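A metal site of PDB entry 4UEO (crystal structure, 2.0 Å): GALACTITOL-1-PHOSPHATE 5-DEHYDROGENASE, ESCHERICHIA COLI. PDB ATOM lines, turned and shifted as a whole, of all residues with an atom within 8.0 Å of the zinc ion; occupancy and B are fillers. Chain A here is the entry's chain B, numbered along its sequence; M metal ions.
Merely in contact with the zinc ion: Phe 90.
Five residues have an atom within 4 Å of the zinc ion: Cys 89, Phe 90, Cys 92, Cys 95 and Cys 103.
SG of Cys 103 sits close to N of Lys 105, 3.6 Å away.
The side-chain sulfur (SG) of Cys 89 sits close to the backbone NH (N) of Thr 91 (3.5 Å).
The side-chain sulfur (SG) of Cys 92 lies close to the backbone NH (N) of Glu 94, 3.6 Å away.
The backbone NH (N) of Phe 90 sits close to the side-chain sulfur (SG) of Cys 95 (3.4 Å).
The side-chain sulfur of Cys 89 lies close to the side-chain amino group of Lys 105 (3.7 Å).
The zinc ion is bound by the side-chain sulfur of Cys 92 (2.3 Å), the side-chain sulfur of Cys 103 (2.4 Å), the side-chain sulfur of Cys 95 (2.4 Å) and the side-chain sulfur of Cys 89 (2.4 Å).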
ATOM      1  N   LEU A  87      -7.587 -25.270  19.299  1.00  0.00           N
ATOM      2  CA  LEU A  87      -8.406 -25.269  18.087  1.00  0.00           C
ATOM      3  C   LEU A  87      -7.962 -24.120  17.175  1.00  0.00           C
ATOM      4  O   LEU A  87      -8.399 -22.997  17.360  1.00  0.00           O
ATOM      5  CB  LEU A  87      -9.897 -25.150  18.440  1.00  0.00           C
ATOM      6  CG  LEU A  87     -10.918 -25.117  17.298  1.00  0.00           C
ATOM      7  CD1 LEU A  87     -10.951 -26.456  16.544  1.00  0.00           C
ATOM      8  CD2 LEU A  87     -12.320 -24.732  17.810  1.00  0.00           C
ATOM      9  N   PRO A  88      -7.064 -24.407  16.219  1.00  0.00           N
ATOM     10  CA  PRO A  88      -6.660 -23.395  15.228  1.00  0.00           C
ATOM     11  C   PRO A  88      -7.740 -23.280  14.167  1.00  0.00           C
ATOM     12  O   PRO A  88      -8.643 -24.113  14.176  1.00  0.00           O
ATOM     13  CB  PRO A  88      -5.371 -23.972  14.640  1.00  0.00           C
ATOM     14  CG  PRO A  88      -5.626 -25.469  14.710  1.00  0.00           C
ATOM     15  CD  PRO A  88      -6.349 -25.680  16.004  1.00  0.00           C
ATOM     16  N   CYS A  89      -7.645 -22.304  13.255  1.00  0.00           N
ATOM     17  CA  CYS A  89      -8.690 -22.119  12.257  1.00  0.00           C
ATOM     18  C   CYS A  89      -8.526 -23.076  11.071  1.00  0.00           C
ATOM     19  O   CYS A  89      -9.458 -23.300  10.305  1.00  0.00           O
ATOM     20  CB  CYS A  89      -8.697 -20.682  11.754  1.00  0.00           C
ATOM     21  SG  CYS A  89      -7.314 -20.307  10.665  1.00  0.00           S
ATOM     22  N   PHE A  90      -7.321 -23.642  10.944  1.00  0.00           N
ATOM     23  CA  PHE A  90      -6.959 -24.614   9.902  1.00  0.00           C
ATOM     24  C   PHE A  90      -6.901 -24.074   8.475  1.00  0.00           C
ATOM     25  O   PHE A  90      -6.504 -24.796   7.561  1.00  0.00           O
ATOM     26  CB  PHE A  90      -7.928 -25.806   9.932  1.00  0.00           C
ATOM     27  CG  PHE A  90      -7.776 -26.658  11.153  1.00  0.00           C
ATOM     28  CD1 PHE A  90      -6.622 -27.393  11.340  1.00  0.00           C
ATOM     29  CD2 PHE A  90      -8.754 -26.675  12.117  1.00  0.00           C
ATOM     30  CE1 PHE A  90      -6.478 -28.163  12.464  1.00  0.00           C
ATOM     31  CE2 PHE A  90      -8.603 -27.444  13.253  1.00  0.00           C
ATOM     32  CZ  PHE A  90      -7.465 -28.196  13.418  1.00  0.00           C
ATOM     33  N   THR A  91      -7.273 -22.823   8.281  1.00  0.00           N
ATOM     34  CA  THR A  91      -7.316 -22.289   6.921  1.00  0.00           C
ATOM     35  C   THR A  91      -6.381 -21.103   6.634  1.00  0.00           C
ATOM     36  O   THR A  91      -6.189 -20.748   5.478  1.00  0.00           O
ATOM     37  CB  THR A  91      -8.744 -21.838   6.570  1.00  0.00           C
ATOM     38  OG1 THR A  91      -9.051 -20.647   7.299  1.00  0.00           O
ATOM     39  CG2 THR A  91      -9.753 -22.916   6.911  1.00  0.00           C
ATOM     40  N   CYS A  92      -5.812 -20.494   7.673  1.00  0.00           N
ATOM     41  CA  CYS A  92      -4.938 -19.328   7.462  1.00  0.00           C
ATOM     42  C   CYS A  92      -3.574 -19.792   6.940  1.00  0.00           C
ATOM     43  O   CYS A  92      -3.265 -20.992   7.009  1.00  0.00           O
ATOM     44  CB  CYS A  92      -4.802 -18.512   8.763  1.00  0.00           C
ATOM     45  SG  CYS A  92      -3.674 -19.266  10.022  1.00  0.00           S
ATOM     46  N   PRO A  93      -2.762 -18.864   6.387  1.00  0.00           N
ATOM     47  CA  PRO A  93      -1.442 -19.263   5.862  1.00  0.00           C
ATOM     48  C   PRO A  93      -0.567 -19.953   6.906  1.00  0.00           C
ATOM     49  O   PRO A  93       0.091 -20.928   6.561  1.00  0.00           O
ATOM     50  CB  PRO A  93      -0.831 -17.927   5.423  1.00  0.00           C
ATOM     51  CG  PRO A  93      -2.069 -17.111   5.002  1.00  0.00           C
ATOM     52  CD  PRO A  93      -3.067 -17.450   6.073  1.00  0.00           C
ATOM     53  N   GLU A  94      -0.574 -19.491   8.144  1.00  0.00           N
ATOM     54  CA  GLU A  94       0.190 -20.187   9.184  1.00  0.00           C
ATOM     55  C   GLU A  94      -0.329 -21.626   9.353  1.00  0.00           C
ATOM     56  O   GLU A  94       0.451 -22.568   9.434  1.00  0.00           O
ATOM     57  CB  GLU A  94       0.124 -19.440  10.532  1.00  0.00           C
ATOM     58  CG  GLU A  94       1.097 -18.275  10.697  1.00  0.00           C
ATOM     59  CD  GLU A  94       0.590 -16.960  10.118  1.00  0.00           C
ATOM     60  OE1 GLU A  94      -0.427 -16.944   9.391  1.00  0.00           O
ATOM     61  OE2 GLU A  94       1.244 -15.931  10.362  1.00  0.00           O
ATOM     62  N   CYS A  95      -1.648 -21.787   9.402  1.00  0.00           N
ATOM     63  CA  CYS A  95      -2.201 -23.121   9.616  1.00  0.00           C
ATOM     64  C   CYS A  95      -1.890 -24.049   8.450  1.00  0.00           C
ATOM     65  O   CYS A  95      -1.603 -25.219   8.648  1.00  0.00           O
ATOM     66  CB  CYS A  95      -3.713 -23.058   9.853  1.00  0.00           C
ATOM     67  SG  CYS A  95      -4.122 -22.770  11.566  1.00  0.00           S
ATOM     68  N   LEU A  96      -1.926 -23.506   7.228  1.00  0.00           N
ATOM     69  CA  LEU A  96      -1.687 -24.321   6.046  1.00  0.00           C
ATOM     70  C   LEU A  96      -0.241 -24.783   5.929  1.00  0.00           C
ATOM     71  O   LEU A  96       0.056 -25.669   5.123  1.00  0.00           O
ATOM     72  CB  LEU A  96      -2.079 -23.550   4.779  1.00  0.00           C
ATOM     73  CG  LEU A  96      -3.566 -23.247   4.559  1.00  0.00           C
ATOM     74  CD1 LEU A  96      -3.717 -22.356   3.316  1.00  0.00           C
ATOM     75  CD2 LEU A  96      -4.398 -24.520   4.406  1.00  0.00           C
ATOM     76  N   PHE A  99       1.796 -24.420  11.014  1.00  0.00           N
ATOM     77  CA  PHE A  99       2.156 -23.563  12.138  1.00  0.00           C
ATOM     78  C   PHE A  99       0.931 -23.303  13.015  1.00  0.00           C
ATOM     79  O   PHE A  99       0.644 -22.153  13.319  1.00  0.00           O
ATOM     80  CB  PHE A  99       2.741 -22.227  11.640  1.00  0.00           C
ATOM     81  CG  PHE A  99       4.041 -22.340  10.878  1.00  0.00           C
ATOM     82  CD1 PHE A  99       4.877 -23.436  11.048  1.00  0.00           C
ATOM     83  CD2 PHE A  99       4.440 -21.326  10.026  1.00  0.00           C
ATOM     84  CE1 PHE A  99       6.101 -23.527  10.350  1.00  0.00           C
ATOM     85  CE2 PHE A  99       5.661 -21.396   9.319  1.00  0.00           C
ATOM     86  CZ  PHE A  99       6.485 -22.499   9.490  1.00  0.00           C
ATOM     87  N   TYR A 100       0.219 -24.358  13.406  1.00  0.00           N
ATOM     88  CA  TYR A 100      -1.012 -24.223  14.180  1.00  0.00           C
ATOM     89  C   TYR A 100      -0.828 -23.350  15.419  1.00  0.00           C
ATOM     90  O   TYR A 100      -1.690 -22.519  15.726  1.00  0.00           O
ATOM     91  CB  TYR A 100      -1.561 -25.598  14.591  1.00  0.00           C
ATOM     92  CG  TYR A 100      -1.651 -26.563  13.437  1.00  0.00           C
ATOM     93  CD1 TYR A 100      -2.553 -26.360  12.419  1.00  0.00           C
ATOM     94  CD2 TYR A 100      -0.805 -27.658  13.363  1.00  0.00           C
ATOM     95  CE1 TYR A 100      -2.629 -27.230  11.347  1.00  0.00           C
ATOM     96  CE2 TYR A 100      -0.870 -28.535  12.293  1.00  0.00           C
ATOM     97  CZ  TYR A 100      -1.788 -28.315  11.301  1.00  0.00           C
ATOM     98  OH  TYR A 100      -1.861 -29.190  10.236  1.00  0.00           O
ATOM     99  N   SER A 101       0.295 -23.515  16.109  1.00  0.00           N
ATOM    100  CA  SER A 101       0.553 -22.745  17.327  1.00  0.00           C
ATOM    101  C   SER A 101       0.787 -21.249  17.059  1.00  0.00           C
ATOM    102  O   SER A 101       0.701 -20.430  17.979  1.00  0.00           O
ATOM    103  CB  SER A 101       1.759 -23.316  18.091  1.00  0.00           C
ATOM    104  OG  SER A 101       2.886 -23.515  17.238  1.00  0.00           O
ATOM    105  N   GLN A 102       1.061 -20.884  15.806  1.00  0.00           N
ATOM    106  CA  GLN A 102       1.138 -19.476  15.437  1.00  0.00           C
ATOM    107  C   GLN A 102      -0.159 -18.970  14.782  1.00  0.00           C
ATOM    108  O   GLN A 102      -0.161 -17.862  14.201  1.00  0.00           O
ATOM    109  CB  GLN A 102       2.307 -19.204  14.474  1.00  0.00           C
ATOM    110  CG  GLN A 102       3.694 -19.263  15.133  1.00  0.00           C
ATOM    111  CD  GLN A 102       4.047 -20.671  15.559  1.00  0.00           C
ATOM    112  OE1 GLN A 102       3.934 -21.607  14.773  1.00  0.00           O
ATOM    113  NE2 GLN A 102       4.458 -20.825  16.808  1.00  0.00           N
ATOM    114  N   CYS A 103      -1.232 -19.741  14.870  1.00  0.00           N
ATOM    115  CA  CYS A 103      -2.527 -19.262  14.352  1.00  0.00           C
ATOM    116  C   CYS A 103      -2.993 -18.085  15.187  1.00  0.00           C
ATOM    117  O   CYS A 103      -2.982 -18.151  16.417  1.00  0.00           O
ATOM    118  CB  CYS A 103      -3.584 -20.387  14.348  1.00  0.00           C
ATOM    119  SG  CYS A 103      -5.243 -19.857  13.665  1.00  0.00           S
ATOM    120  N   ALA A 104      -3.422 -17.016  14.524  1.00  0.00           N
ATOM    121  CA  ALA A 104      -3.834 -15.785  15.215  1.00  0.00           C
ATOM    122  C   ALA A 104      -5.209 -15.905  15.856  1.00  0.00           C
ATOM    123  O   ALA A 104      -5.484 -15.278  16.879  1.00  0.00           O
ATOM    124  CB  ALA A 104      -3.821 -14.622  14.244  1.00  0.00           C
ATOM    125  N   LYS A 105      -6.088 -16.709  15.252  1.00  0.00           N
ATOM    126  CA  LYS A 105      -7.442 -16.872  15.766  1.00  0.00           C
ATOM    127  C   LYS A 105      -7.586 -18.252  16.379  1.00  0.00           C
ATOM    128  O   LYS A 105      -8.431 -19.036  15.954  1.00  0.00           O
ATOM    129  CB  LYS A 105      -8.475 -16.686  14.657  1.00  0.00           C
ATOM    130  CG  LYS A 105      -8.261 -15.440  13.818  1.00  0.00           C
ATOM    131  CD  LYS A 105      -8.788 -15.666  12.405  1.00  0.00           C
ATOM    132  CE  LYS A 105      -8.162 -16.915  11.770  1.00  0.00           C
ATOM    133  NZ  LYS A 105      -6.706 -16.778  11.473  1.00  0.00           N
ATOM    134  N   TYR A 106      -6.754 -18.534  17.374  1.00  0.00           N
ATOM    135  CA  TYR A 106      -6.776 -19.825  18.034  1.00  0.00           C
ATOM    136  C   TYR A 106      -7.987 -19.951  18.950  1.00  0.00           C
ATOM    137  O   TYR A 106      -8.835 -19.054  19.029  1.00  0.00           O
ATOM    138  CB  TYR A 106      -5.483 -20.042  18.847  1.00  0.00           C
ATOM    139  CG  TYR A 106      -5.293 -19.055  19.968  1.00  0.00           C
ATOM    140  CD1 TYR A 106      -4.627 -17.850  19.762  1.00  0.00           C
ATOM    141  CD2 TYR A 106      -5.776 -19.320  21.254  1.00  0.00           C
ATOM    142  CE1 TYR A 106      -4.455 -16.937  20.791  1.00  0.00           C
ATOM    143  CE2 TYR A 106      -5.603 -18.421  22.285  1.00  0.00           C
ATOM    144  CZ  TYR A 106      -4.933 -17.226  22.051  1.00  0.00           C
ATOM    145  OH  TYR A 106      -4.768 -16.329  23.070  1.00  0.00           O
HETATM  146 ZN    ZN M   1      -5.041 -20.569  11.393  1.00  0.00          ZN
